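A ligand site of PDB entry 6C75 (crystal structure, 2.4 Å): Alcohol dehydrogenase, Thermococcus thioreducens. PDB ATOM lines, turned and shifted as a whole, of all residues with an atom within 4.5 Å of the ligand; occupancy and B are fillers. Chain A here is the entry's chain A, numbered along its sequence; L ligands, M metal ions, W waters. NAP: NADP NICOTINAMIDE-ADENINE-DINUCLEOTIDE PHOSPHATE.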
ATOM      1  N   SER A  33      12.635   5.272 -15.511  1.00  0.00           N
ATOM      2  CA  SER A  33      14.074   5.388 -15.283  1.00  0.00           C
ATOM      3  C   SER A  33      14.738   4.017 -15.235  1.00  0.00           C
ATOM      4  O   SER A  33      14.108   3.015 -14.886  1.00  0.00           O
ATOM      5  CB  SER A  33      14.334   6.135 -13.981  1.00  0.00           C
ATOM      6  OG  SER A  33      14.024   5.308 -12.872  1.00  0.00           O
ATOM      7  N   GLY A  34      16.036   3.985 -15.522  1.00  0.00           N
ATOM      8  CA  GLY A  34      16.786   2.752 -15.516  1.00  0.00           C
ATOM      9  C   GLY A  34      16.636   1.986 -14.217  1.00  0.00           C
ATOM     10  O   GLY A  34      16.497   0.762 -14.218  1.00  0.00           O
ATOM     11  N   SER A  35      16.697   2.706 -13.095  1.00  0.00           N
ATOM     12  CA  SER A  35      16.683   2.072 -11.782  1.00  0.00           C
ATOM     13  C   SER A  35      15.387   1.294 -11.522  1.00  0.00           C
ATOM     14  O   SER A  35      15.399   0.292 -10.829  1.00  0.00           O
ATOM     15  CB  SER A  35      16.870   3.126 -10.688  1.00  0.00           C
ATOM     16  OG  SER A  35      16.048   4.252 -10.940  1.00  0.00           O
ATOM     17  N   MET A  36      14.281   1.777 -12.071  1.00  0.00           N
ATOM     18  CA  MET A  36      12.988   1.146 -11.831  1.00  0.00           C
ATOM     19  C   MET A  36      12.913  -0.229 -12.473  1.00  0.00           C
ATOM     20  O   MET A  36      12.259  -1.133 -11.944  1.00  0.00           O
ATOM     21  CB  MET A  36      11.856   2.032 -12.367  1.00  0.00           C
ATOM     22  CG  MET A  36      11.635   3.320 -11.579  1.00  0.00           C
ATOM     23  SD  MET A  36      11.034   3.012  -9.902  1.00  0.00           S
ATOM     24  CE  MET A  36      12.571   3.077  -8.977  1.00  0.00           C
ATOM     25  N   ARG A  38      15.866  -2.057 -12.891  1.00  0.00           N
ATOM     26  CA  ARG A  38      16.855  -2.826 -12.119  1.00  0.00           C
ATOM     27  C   ARG A  38      16.280  -3.377 -10.819  1.00  0.00           C
ATOM     28  O   ARG A  38      16.755  -4.387 -10.300  1.00  0.00           O
ATOM     29  CB  ARG A  38      18.078  -1.975 -11.805  1.00  0.00           C
ATOM     30  CG  ARG A  38      19.017  -1.761 -12.988  1.00  0.00           C
ATOM     31  CD  ARG A  38      20.420  -1.355 -12.536  1.00  0.00           C
ATOM     32  NE  ARG A  38      20.444  -0.039 -11.915  1.00  0.00           N
ATOM     33  CZ  ARG A  38      20.327   1.113 -12.582  1.00  0.00           C
ATOM     34  NH1 ARG A  38      20.155   1.118 -13.900  1.00  0.00           N
ATOM     35  NH2 ARG A  38      20.336   2.272 -11.917  1.00  0.00           N
ATOM     36  N   LEU A  62      15.407   6.511 -19.435  1.00  0.00           N
ATOM     37  CA  LEU A  62      15.351   7.946 -19.685  1.00  0.00           C
ATOM     38  C   LEU A  62      16.436   8.659 -18.876  1.00  0.00           C
ATOM     39  O   LEU A  62      16.621   8.376 -17.698  1.00  0.00           O
ATOM     40  CB  LEU A  62      13.967   8.481 -19.312  1.00  0.00           C
ATOM     41  CG  LEU A  62      12.989   8.673 -20.461  1.00  0.00           C
ATOM     42  CD1 LEU A  62      12.968   7.482 -21.408  1.00  0.00           C
ATOM     43  CD2 LEU A  62      11.598   8.947 -19.920  1.00  0.00           C
ATOM     44  N   ALA A  64      18.624  11.440 -16.759  1.00  0.00           N
ATOM     45  CA  ALA A  64      18.468  12.506 -15.769  1.00  0.00           C
ATOM     46  C   ALA A  64      18.733  13.874 -16.406  1.00  0.00           C
ATOM     47  O   ALA A  64      19.453  13.977 -17.397  1.00  0.00           O
ATOM     48  CB  ALA A  64      19.403  12.278 -14.595  1.00  0.00           C
ATOM     49  N   GLU A  65      18.164  14.910 -15.800  1.00  0.00           N
ATOM     50  CA  GLU A  65      18.332  16.298 -16.271  1.00  0.00           C
ATOM     51  C   GLU A  65      18.219  16.393 -17.792  1.00  0.00           C
ATOM     52  O   GLU A  65      19.167  16.853 -18.449  1.00  0.00           O
ATOM     53  CB  GLU A  65      19.677  16.866 -15.824  1.00  0.00           C
ATOM     54  CG  GLU A  65      20.001  16.632 -14.347  1.00  0.00           C
ATOM     55  CD  GLU A  65      19.683  17.840 -13.486  1.00  0.00           C
ATOM     56  OE1 GLU A  65      20.146  18.949 -13.821  1.00  0.00           O
ATOM     57  OE2 GLU A  65      19.037  17.660 -12.428  1.00  0.00           O
ATOM     58  N   PRO A  66      17.034  16.077 -18.338  1.00  0.00           N
ATOM     59  CA  PRO A  66      16.848  15.955 -19.782  1.00  0.00           C
ATOM     60  C   PRO A  66      17.079  17.272 -20.527  1.00  0.00           C
ATOM     61  O   PRO A  66      16.805  18.347 -19.996  1.00  0.00           O
ATOM     62  CB  PRO A  66      15.387  15.522 -19.909  1.00  0.00           C
ATOM     63  CG  PRO A  66      14.722  16.119 -18.721  1.00  0.00           C
ATOM     64  CD  PRO A  66      15.747  16.137 -17.623  1.00  0.00           C
ATOM     65  N   GLY A  91      12.160   9.665 -11.395  1.00  0.00           N
ATOM     66  CA  GLY A  91      12.288  10.954 -10.733  1.00  0.00           C
ATOM     67  C   GLY A  91      11.746  12.066 -11.604  1.00  0.00           C
ATOM     68  O   GLY A  91      11.117  11.814 -12.632  1.00  0.00           O
ATOM     69  N   GLY A  92      11.993  13.309 -11.190  1.00  0.00           N
ATOM     70  CA  GLY A  92      11.425  14.477 -11.872  1.00  0.00           C
ATOM     71  C   GLY A  92      11.821  14.557 -13.325  1.00  0.00           C
ATOM     72  O   GLY A  92      11.030  14.947 -14.182  1.00  0.00           O
ATOM     73  N   SER A  93      13.075  14.206 -13.622  1.00  0.00           N
ATOM     74  CA  SER A  93      13.538  14.191 -14.993  1.00  0.00           C
ATOM     75  C   SER A  93      12.606  13.391 -15.890  1.00  0.00           C
ATOM     76  O   SER A  93      12.292  13.808 -16.993  1.00  0.00           O
ATOM     77  CB  SER A  93      14.948  13.596 -15.036  1.00  0.00           C
ATOM     78  OG  SER A  93      15.837  14.399 -14.298  1.00  0.00           O
ATOM     79  N   VAL A  94      12.220  12.212 -15.418  1.00  0.00           N
ATOM     80  CA  VAL A  94      11.437  11.283 -16.239  1.00  0.00           C
ATOM     81  C   VAL A  94      10.007  11.793 -16.392  1.00  0.00           C
ATOM     82  O   VAL A  94       9.439  11.762 -17.486  1.00  0.00           O
ATOM     83  CB  VAL A  94      11.419   9.879 -15.602  1.00  0.00           C
ATOM     84  CG1 VAL A  94      10.377   8.999 -16.300  1.00  0.00           C
ATOM     85  CG2 VAL A  94      12.790   9.235 -15.681  1.00  0.00           C
ATOM     86  N   ASP A  96       9.046  14.874 -16.225  1.00  0.00           N
ATOM     87  CA  ASP A  96       9.068  16.067 -17.067  1.00  0.00           C
ATOM     88  C   ASP A  96       9.133  15.696 -18.549  1.00  0.00           C
ATOM     89  O   ASP A  96       8.548  16.373 -19.396  1.00  0.00           O
ATOM     90  CB  ASP A  96      10.271  16.943 -16.703  1.00  0.00           C
ATOM     91  CG  ASP A  96       9.997  17.829 -15.513  1.00  0.00           C
ATOM     92  OD1 ASP A  96       8.920  17.665 -14.898  1.00  0.00           O
ATOM     93  OD2 ASP A  96      10.834  18.701 -15.205  1.00  0.00           O
ATOM     94  N   LYS A  99       5.813  14.533 -19.578  1.00  0.00           N
ATOM     95  CA  LYS A  99       5.001  15.741 -19.715  1.00  0.00           C
ATOM     96  C   LYS A  99       5.218  16.389 -21.072  1.00  0.00           C
ATOM     97  O   LYS A  99       4.271  16.762 -21.747  1.00  0.00           O
ATOM     98  CB  LYS A  99       5.356  16.742 -18.615  1.00  0.00           C
ATOM     99  CG  LYS A  99       4.615  16.552 -17.303  1.00  0.00           C
ATOM    100  CD  LYS A  99       4.955  17.688 -16.353  1.00  0.00           C
ATOM    101  CE  LYS A  99       4.463  17.404 -14.936  1.00  0.00           C
ATOM    102  NZ  LYS A  99       5.014  18.394 -13.968  1.00  0.00           N
ATOM    103  N   SER A 139       9.811   8.380  -7.868  1.00  0.00           N
ATOM    104  CA  SER A 139      10.649   7.378  -7.210  1.00  0.00           C
ATOM    105  C   SER A 139      11.762   8.047  -6.427  1.00  0.00           C
ATOM    106  O   SER A 139      12.485   7.391  -5.680  1.00  0.00           O
ATOM    107  CB  SER A 139      11.224   6.409  -8.234  1.00  0.00           C
ATOM    108  OG  SER A 139      11.943   7.095  -9.243  1.00  0.00           O
ATOM    109  N   THR A 140      11.892   9.358  -6.598  1.00  0.00           N
ATOM    110  CA  THR A 140      12.686  10.184  -5.684  1.00  0.00           C
ATOM    111  C   THR A 140      11.789  11.048  -4.796  1.00  0.00           C
ATOM    112  O   THR A 140      10.585  11.151  -5.023  1.00  0.00           O
ATOM    113  CB  THR A 140      13.630  11.122  -6.472  1.00  0.00           C
ATOM    114  OG1 THR A 140      12.855  12.096  -7.174  1.00  0.00           O
ATOM    115  CG2 THR A 140      14.461  10.337  -7.480  1.00  0.00           C
ATOM    116  N   ALA A 143      11.098  16.038  -6.640  1.00  0.00           N
ATOM    117  CA  ALA A 143      11.053  17.270  -7.417  1.00  0.00           C
ATOM    118  C   ALA A 143       9.662  17.920  -7.378  1.00  0.00           C
ATOM    119  O   ALA A 143       9.530  19.097  -7.707  1.00  0.00           O
ATOM    120  CB  ALA A 143      11.448  17.004  -8.859  1.00  0.00           C
ATOM    121  N   GLY A 144       8.647  17.126  -7.044  1.00  0.00           N
ATOM    122  CA  GLY A 144       7.282  17.645  -6.941  1.00  0.00           C
ATOM    123  C   GLY A 144       6.616  17.800  -8.306  1.00  0.00           C
ATOM    124  O   GLY A 144       5.492  18.288  -8.409  1.00  0.00           O
ATOM    125  N   SER A 145       7.267  17.283  -9.332  1.00  0.00           N
ATOM    126  CA  SER A 145       6.755  17.401 -10.693  1.00  0.00           C
ATOM    127  C   SER A 145       5.486  16.586 -10.894  1.00  0.00           C
ATOM    128  O   SER A 145       4.767  16.763 -11.873  1.00  0.00           O
ATOM    129  CB  SER A 145       7.818  16.940 -11.682  1.00  0.00           C
ATOM    130  OG  SER A 145       7.287  16.926 -12.991  1.00  0.00           O
ATOM    131  N   SER A 148       2.859  19.262 -10.384  1.00  0.00           N
ATOM    132  CA  SER A 148       3.080  20.582 -10.952  1.00  0.00           C
ATOM    133  C   SER A 148       2.628  20.639 -12.412  1.00  0.00           C
ATOM    134  O   SER A 148       2.454  19.590 -13.045  1.00  0.00           O
ATOM    135  CB  SER A 148       4.560  20.963 -10.858  1.00  0.00           C
ATOM    136  OG  SER A 148       5.242  20.620 -12.040  1.00  0.00           O
ATOM    137  N   ALA A 150       4.485  22.252 -14.671  1.00  0.00           N
ATOM    138  CA  ALA A 150       5.685  22.691 -15.352  1.00  0.00           C
ATOM    139  C   ALA A 150       6.465  21.498 -15.885  1.00  0.00           C
ATOM    140  O   ALA A 150       6.340  20.389 -15.386  1.00  0.00           O
ATOM    141  CB  ALA A 150       6.547  23.524 -14.420  1.00  0.00           C
ATOM    142  N   VAL A 152      10.674  21.084 -17.217  1.00  0.00           N
ATOM    143  CA  VAL A 152      11.936  21.822 -17.278  1.00  0.00           C
ATOM    144  C   VAL A 152      12.907  21.087 -18.185  1.00  0.00           C
ATOM    145  O   VAL A 152      13.426  20.024 -17.827  1.00  0.00           O
ATOM    146  CB  VAL A 152      12.563  21.966 -15.877  1.00  0.00           C
ATOM    147  CG1 VAL A 152      13.601  23.071 -15.876  1.00  0.00           C
ATOM    148  CG2 VAL A 152      11.491  22.238 -14.827  1.00  0.00           C
ATOM    149  N   LYS A 159      18.226  25.851 -18.105  1.00  0.00           N
ATOM    150  CA  LYS A 159      16.885  25.324 -17.870  1.00  0.00           C
ATOM    151  C   LYS A 159      15.806  26.368 -18.168  1.00  0.00           C
ATOM    152  O   LYS A 159      15.925  27.526 -17.746  1.00  0.00           O
ATOM    153  CB  LYS A 159      16.755  24.810 -16.440  1.00  0.00           C
ATOM    154  CG  LYS A 159      17.073  23.331 -16.284  1.00  0.00           C
ATOM    155  CD  LYS A 159      17.860  23.048 -15.004  1.00  0.00           C
ATOM    156  CE  LYS A 159      17.410  21.748 -14.342  1.00  0.00           C
ATOM    157  NZ  LYS A 159      17.882  20.550 -15.085  1.00  0.00           N
ATOM    158  N   LEU A 178       9.366   2.688  -3.541  1.00  0.00           N
ATOM    159  CA  LEU A 178      10.216   3.135  -4.645  1.00  0.00           C
ATOM    160  C   LEU A 178      11.410   3.960  -4.155  1.00  0.00           C
ATOM    161  O   LEU A 178      12.564   3.569  -4.366  1.00  0.00           O
ATOM    162  CB  LEU A 178       9.403   3.892  -5.689  1.00  0.00           C
ATOM    163  CG  LEU A 178       8.747   3.003  -6.755  1.00  0.00           C
ATOM    164  CD1 LEU A 178       7.904   1.914  -6.128  1.00  0.00           C
ATOM    165  CD2 LEU A 178       7.903   3.830  -7.716  1.00  0.00           C
ATOM    166  N   PRO A 179      11.155   5.054  -3.435  1.00  0.00           N
ATOM    167  CA  PRO A 179      12.279   5.905  -3.012  1.00  0.00           C
ATOM    168  C   PRO A 179      13.239   5.219  -2.036  1.00  0.00           C
ATOM    169  O   PRO A 179      14.343   5.722  -1.786  1.00  0.00           O
ATOM    170  CB  PRO A 179      11.595   7.110  -2.362  1.00  0.00           C
ATOM    171  CG  PRO A 179      10.198   6.684  -2.076  1.00  0.00           C
ATOM    172  CD  PRO A 179       9.854   5.681  -3.146  1.00  0.00           C
ATOM    173  N   THR A 181      14.986   2.736  -2.502  1.00  0.00           N
ATOM    174  CA  THR A 181      16.163   2.260  -3.226  1.00  0.00           C
ATOM    175  C   THR A 181      17.068   3.400  -3.698  1.00  0.00           C
ATOM    176  O   THR A 181      18.119   3.144  -4.283  1.00  0.00           O
ATOM    177  CB  THR A 181      15.755   1.403  -4.441  1.00  0.00           C
ATOM    178  OG1 THR A 181      15.127   2.218  -5.433  1.00  0.00           O
ATOM    179  CG2 THR A 181      14.808   0.289  -4.030  1.00  0.00           C
ATOM    180  N   MET A 182      16.704   4.646  -3.406  1.00  0.00           N
ATOM    181  CA  MET A 182      17.594   5.775  -3.666  1.00  0.00           C
ATOM    182  C   MET A 182      18.913   5.569  -2.950  1.00  0.00           C
ATOM    183  O   MET A 182      18.939   5.496  -1.719  1.00  0.00           O
ATOM    184  CB  MET A 182      16.971   7.088  -3.172  1.00  0.00           C
ATOM    185  CG  MET A 182      15.995   7.748  -4.140  1.00  0.00           C
ATOM    186  SD  MET A 182      15.502   9.391  -3.590  1.00  0.00           S
ATOM    187  CE  MET A 182      14.845   9.031  -1.966  1.00  0.00           C
ATOM    188  N   PRO A 183      20.028   5.637  -3.695  1.00  0.00           N
ATOM    189  CA  PRO A 183      21.330   5.835  -3.060  1.00  0.00           C
ATOM    190  C   PRO A 183      21.392   7.166  -2.325  1.00  0.00           C
ATOM    191  O   PRO A 183      20.718   8.103  -2.737  1.00  0.00           O
ATOM    192  CB  PRO A 183      22.306   5.804  -4.229  1.00  0.00           C
ATOM    193  CG  PRO A 183      21.503   6.172  -5.421  1.00  0.00           C
ATOM    194  CD  PRO A 183      20.128   5.629  -5.166  1.00  0.00           C
ATOM    195  N   VAL A 186      21.425  10.729  -3.963  1.00  0.00           N
ATOM    196  CA  VAL A 186      20.156  11.063  -4.611  1.00  0.00           C
ATOM    197  C   VAL A 186      19.114  11.452  -3.579  1.00  0.00           C
ATOM    198  O   VAL A 186      18.347  12.390  -3.780  1.00  0.00           O
ATOM    199  CB  VAL A 186      19.628   9.877  -5.438  1.00  0.00           C
ATOM    200  CG1 VAL A 186      18.219  10.180  -5.934  1.00  0.00           C
ATOM    201  CG2 VAL A 186      20.551   9.586  -6.616  1.00  0.00           C
ATOM    202  N   SER A 190      17.684  15.335  -3.755  1.00  0.00           N
ATOM    203  CA  SER A 190      16.265  15.529  -3.989  1.00  0.00           C
ATOM    204  C   SER A 190      15.572  15.963  -2.690  1.00  0.00           C
ATOM    205  O   SER A 190      14.597  16.719  -2.717  1.00  0.00           O
ATOM    206  CB  SER A 190      15.629  14.255  -4.554  1.00  0.00           C
ATOM    207  OG  SER A 190      15.542  13.242  -3.574  1.00  0.00           O
ATOM    208  N   ASP A 193      16.005  19.691  -2.131  1.00  0.00           N
ATOM    209  CA  ASP A 193      15.095  20.358  -3.048  1.00  0.00           C
ATOM    210  C   ASP A 193      13.731  20.612  -2.393  1.00  0.00           C
ATOM    211  O   ASP A 193      13.207  21.719  -2.450  1.00  0.00           O
ATOM    212  CB  ASP A 193      14.925  19.494  -4.298  1.00  0.00           C
ATOM    213  CG  ASP A 193      14.739  20.301  -5.565  1.00  0.00           C
ATOM    214  OD1 ASP A 193      14.866  21.547  -5.504  1.00  0.00           O
ATOM    215  OD2 ASP A 193      14.538  19.677  -6.622  1.00  0.00           O
ATOM    216  N   HIS A 197      12.135  24.266  -1.906  1.00  0.00           N
ATOM    217  CA  HIS A 197      10.760  24.496  -2.361  1.00  0.00           C
ATOM    218  C   HIS A 197       9.891  25.082  -1.243  1.00  0.00           C
ATOM    219  O   HIS A 197       9.095  26.005  -1.487  1.00  0.00           O
ATOM    220  CB  HIS A 197      10.134  23.196  -2.839  1.00  0.00           C
ATOM    221  CG  HIS A 197      10.670  22.717  -4.156  1.00  0.00           C
ATOM    222  ND1 HIS A 197      10.636  21.385  -4.523  1.00  0.00           N
ATOM    223  CD2 HIS A 197      11.289  23.383  -5.155  1.00  0.00           C
ATOM    224  CE1 HIS A 197      11.238  21.252  -5.695  1.00  0.00           C
ATOM    225  NE2 HIS A 197      11.619  22.445  -6.106  1.00  0.00           N
ATOM    226  N   PHE A 251       4.157  24.899  -4.230  1.00  0.00           N
ATOM    227  CA  PHE A 251       4.798  25.742  -5.239  1.00  0.00           C
ATOM    228  C   PHE A 251       4.082  25.669  -6.601  1.00  0.00           C
ATOM    229  O   PHE A 251       4.116  26.627  -7.353  1.00  0.00           O
ATOM    230  CB  PHE A 251       6.304  25.453  -5.351  1.00  0.00           C
ATOM    231  CG  PHE A 251       6.672  24.324  -6.267  1.00  0.00           C
ATOM    232  CD1 PHE A 251       6.509  24.441  -7.641  1.00  0.00           C
ATOM    233  CD2 PHE A 251       7.435  23.256  -5.801  1.00  0.00           C
ATOM    234  CE1 PHE A 251       6.844  23.395  -8.487  1.00  0.00           C
ATOM    235  CE2 PHE A 251       7.792  22.218  -6.642  1.00  0.00           C
ATOM    236  CZ  PHE A 251       7.493  22.284  -7.984  1.00  0.00           C
ATOM    237  N   HIS A 260      15.769  29.193  -7.293  1.00  0.00           N
ATOM    238  CA  HIS A 260      15.481  28.277  -8.379  1.00  0.00           C
ATOM    239  C   HIS A 260      15.867  28.874  -9.721  1.00  0.00           C
ATOM    240  O   HIS A 260      16.341  28.160 -10.607  1.00  0.00           O
ATOM    241  CB  HIS A 260      14.011  27.885  -8.389  1.00  0.00           C
ATOM    242  CG  HIS A 260      13.742  26.555  -7.749  1.00  0.00           C
ATOM    243  ND1 HIS A 260      13.915  26.339  -6.398  1.00  0.00           N
ATOM    244  CD2 HIS A 260      13.486  25.347  -8.305  1.00  0.00           C
ATOM    245  CE1 HIS A 260      13.734  25.057  -6.143  1.00  0.00           C
ATOM    246  NE2 HIS A 260      13.445  24.444  -7.273  1.00  0.00           N
ATOM    247  N   HIS A 272      20.391  19.539  -9.787  1.00  0.00           N
ATOM    248  CA  HIS A 272      19.473  20.614  -9.403  1.00  0.00           C
ATOM    249  C   HIS A 272      19.381  20.791  -7.886  1.00  0.00           C
ATOM    250  O   HIS A 272      19.400  21.920  -7.392  1.00  0.00           O
ATOM    251  CB  HIS A 272      18.086  20.294  -9.958  1.00  0.00           C
ATOM    252  CG  HIS A 272      17.057  21.321  -9.620  1.00  0.00           C
ATOM    253  ND1 HIS A 272      17.014  22.555 -10.223  1.00  0.00           N
ATOM    254  CD2 HIS A 272      16.027  21.285  -8.740  1.00  0.00           C
ATOM    255  CE1 HIS A 272      15.986  23.235  -9.750  1.00  0.00           C
ATOM    256  NE2 HIS A 272      15.359  22.487  -8.866  1.00  0.00           N
HETATM  257  PA  NAP L   1      16.149  12.752 -11.295  1.00  0.00           P
HETATM  258  O1A NAP L   1      17.030  13.776 -11.977  1.00  0.00           O
HETATM  259  O2A NAP L   1      14.802  12.397 -11.901  1.00  0.00           O
HETATM  260  O5B NAP L   1      17.019  11.408 -11.170  1.00  0.00           O
HETATM  261  C5B NAP L   1      18.295  11.490 -10.539  1.00  0.00           C
HETATM  262  C4B NAP L   1      18.960  10.124 -10.439  1.00  0.00           C
HETATM  263  O4B NAP L   1      18.350   9.349  -9.408  1.00  0.00           O
HETATM  264  C3B NAP L   1      18.855   9.314 -11.721  1.00  0.00           C
HETATM  265  O3B NAP L   1      20.151   9.178 -12.318  1.00  0.00           O
HETATM  266  C2B NAP L   1      18.314   7.954 -11.322  1.00  0.00           C
HETATM  267  O2B NAP L   1      19.141   6.911 -11.821  1.00  0.00           O
HETATM  268  C1B NAP L   1      18.289   7.978  -9.794  1.00  0.00           C
HETATM  269  N9A NAP L   1      17.085   7.343  -9.216  1.00  0.00           N
HETATM  270  C8A NAP L   1      15.832   7.843  -9.229  1.00  0.00           C
HETATM  271  N7A NAP L   1      15.001   7.065  -8.503  1.00  0.00           N
HETATM  272  C5A NAP L   1      15.745   6.096  -7.920  1.00  0.00           C
HETATM  273  C6A NAP L   1      15.489   4.912  -7.075  1.00  0.00           C
HETATM  274  N6A NAP L   1      14.257   4.644  -6.580  1.00  0.00           N
HETATM  275  N1A NAP L   1      16.542   4.112  -6.762  1.00  0.00           N
HETATM  276  C2A NAP L   1      17.782   4.362  -7.234  1.00  0.00           C
HETATM  277  N3A NAP L   1      18.074   5.395  -8.032  1.00  0.00           N
HETATM  278  C4A NAP L   1      17.125   6.294  -8.393  1.00  0.00           C
HETATM  279  O3  NAP L   1      15.957  13.178  -9.732  1.00  0.00           O
HETATM  280  PN  NAP L   1      14.996  14.371  -9.212  1.00  0.00           P
HETATM  281  O1N NAP L   1      13.639  13.796  -8.902  1.00  0.00           O
HETATM  282  O2N NAP L   1      15.707  15.163  -8.145  1.00  0.00           O
HETATM  283  O5D NAP L   1      14.841  15.254 -10.561  1.00  0.00           O
HETATM  284  C5D NAP L   1      15.159  16.627 -10.659  1.00  0.00           C
HETATM  285  C4D NAP L   1      14.681  17.120 -12.021  1.00  0.00           C
HETATM  286  O4D NAP L   1      13.327  17.595 -11.910  1.00  0.00           O
HETATM  287  C3D NAP L   1      15.526  18.269 -12.568  1.00  0.00           C
HETATM  288  O3D NAP L   1      15.849  18.050 -13.947  1.00  0.00           O
HETATM  289  C2D NAP L   1      14.663  19.507 -12.414  1.00  0.00           C
HETATM  290  O2D NAP L   1      14.819  20.385 -13.530  1.00  0.00           O
HETATM  291  C1D NAP L   1      13.248  18.957 -12.337  1.00  0.00           C
HETATM  292  N1N NAP L   1      12.388  19.734 -11.436  1.00  0.00           N
HETATM  293  C2N NAP L   1      11.106  19.879 -11.794  1.00  0.00           C
HETATM  294  C3N NAP L   1      10.238  20.652 -11.046  1.00  0.00           C
HETATM  295  C7N NAP L   1       8.813  20.797 -11.505  1.00  0.00           C
HETATM  296  O7N NAP L   1       7.968  21.258 -10.757  1.00  0.00           O
HETATM  297  N7N NAP L   1       8.495  20.403 -12.737  1.00  0.00           N
HETATM  298  C4N NAP L   1      10.709  21.293  -9.909  1.00  0.00           C
HETATM  299  C5N NAP L   1      12.040  21.111  -9.541  1.00  0.00           C
HETATM  300  C6N NAP L   1      12.872  20.330 -10.333  1.00  0.00           C
HETATM  301  P2B NAP L   1      18.735   6.125 -13.175  1.00  0.00           P
HETATM  302  O1X NAP L   1      18.584   7.207 -14.205  1.00  0.00           O
HETATM  303  O2X NAP L   1      19.900   5.197 -13.421  1.00  0.00           O
HETATM  304  O3X NAP L   1      17.453   5.420 -12.808  1.00  0.00           O
HETATM  305 FE    FE M   1      13.410  22.207  -7.265  1.00  0.00          FE
HETATM  306  O   HOH W   1      14.900   9.498 -12.364  1.00  0.00           O
HETATM  307  O   HOH W   2      16.393   9.260 -14.706  1.00  0.00           O
HETATM  308  O   HOH W   3      17.382   6.020 -16.291  1.00  0.00           O
HETATM  309  O   HOH W   4      18.107  16.945  -7.856  1.00  0.00           O
HETATM  310  O   HOH W   5      19.321  15.011 -10.968  1.00  0.00           O
HETATM  311  O   HOH W   6      13.424  18.025 -15.528  1.00  0.00           O
HETATM  312  O   HOH W   7      22.129   6.105 -10.867  1.00  0.00           O
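Water W3 lies within hydrogen-bond range of N of Gly 34 (2.6 Å), O1X of the ligand (2.7 Å) and O of Leu 62 (2.8 Å).
Water W5 bridges O1A of the ligand (2.8 Å) and OE2 of Glu 65 (3.0 Å).
Water W6 lies within hydrogen-bond range of the side-chain carboxylate of Asp 96 (2.7 Å), an oxygen (O3D) of the ligand (2.9 Å) and the backbone carbonyl oxygen of Val 152 (3.0 Å).
Water W1 bridges the backbone NH of Gly 91 (2.9 Å) and an oxygen (O2A) of the ligand (2.9 Å).
Water W2 bridges O1X of the ligand and O of Leu 62.
Met 36 touches the ligand.
Ala 64 touches the ligand.
OE2 of Glu 65 touches O3D of the ligand (3.6 Å).
Gly 91 touches the ligand.
OD1 of Asp 96 touches N7N of the ligand (3.5 Å).
Ala 143 touches the ligand (O to C4N, 3.3 Å).
Ser 145 touches the ligand (CB to N7N, 3.7 Å).
CB of Val 152 touches O2D of the ligand, at 3.6 Å.
Pro 183 touches the ligand (CD to C2A, 3.4 Å).
Val 186 touches the ligand.
Ser 190 touches the ligand.
His 197 touches the ligand (NE2 to C5N, 3.7 Å).
Phe 251 touches the ligand.
His 272 touches the ligand.
Of the 36 residues printed, 28 come within 4 Å of the ligand.
Along chain A the residues within 4 Å of the ligand span positions 33 to 272.
An oxygen (O1N) of the ligand sits at hydrogen-bond distance from the side-chain hydroxyl (OG1) of Thr 140.
N of Ser 35 sits at hydrogen-bond distance from O3X of the ligand, 2.8 Å away.
O3X of the ligand is in hydrogen-bond range of OG of Ser 35, at 2.6 Å.
O2A of the ligand sits at hydrogen-bond distance from N of Ser 93 (3.0 Å).
OG of Ser 93 sits at hydrogen-bond distance from O1A of the ligand, at 2.7 Å.
The side-chain hydroxyl (OG1) of Thr 181 lies within hydrogen-bond range of a nitrogen (N1A) of the ligand.
The backbone NH (N) of Gly 92 is in hydrogen-bond range of an oxygen (O1N) of the ligand.
O of Leu 178 is in hydrogen-bond range of N6A of the ligand (3.0 Å).
An oxygen (O3D) of the ligand is in hydrogen-bond range of the side-chain amino group of Lys 159.
O7N of the ligand lies within hydrogen-bond range of OG of Ser 148, 3.1 Å away.
The backbone carbonyl oxygen of Ser 139 sits at hydrogen-bond distance from a nitrogen (N6A) of the ligand, at 3.4 Å.
OG of Ser 139 lies within hydrogen-bond range of N7A of the ligand, at 3.1 Å.
NH2 of Arg 38 is in salt-bridge range of O2X of the ligand, 3.3 Å away.
An oxygen (O3X) of the ligand sits at hydrogen-bond distance from the backbone NH (N) of Gly 34 (3.4 Å).
N of Met 182 sits at hydrogen-bond distance from N1A of the ligand (3.4 Å).
The side-chain hydroxyl (OG) of Ser 33 lies close to an oxygen (O3X) of the ligand.
The backbone carbonyl oxygen of Ala 150 lies within hydrogen-bond range of a nitrogen (N7N) of the ligand.
The side-chain hydroxyl (OG) of Ser 35 lies within hydrogen-bond range of the side-chain hydroxyl (OG) of Ser 33, 3.0 Å away.
O of Leu 178 lies within hydrogen-bond range of OG1 of Thr 181, 3.1 Å away.
The side-chain amino group (NZ) of Lys 159 lies within salt-bridge range of the side-chain carboxylate (OE1) of Glu 65 (3.0 Å).
NZ of Lys 99 sits at hydrogen-bond distance from OG of Ser 148 (3.0 Å).
The side-chain hydroxyl (OG) of Ser 139 sits at hydrogen-bond distance from the backbone NH (N) of Gly 91.
The side-chain amino group (NZ) of Lys 99 is in hydrogen-bond range of the backbone carbonyl oxygen (O) of Ala 150 (2.8 Å).
The side-chain carboxylate of Asp 96 lies within hydrogen-bond range of the backbone NH of Val 152.
O of Val 186 lies within hydrogen-bond range of OG of Ser 190 (2.9 Å).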
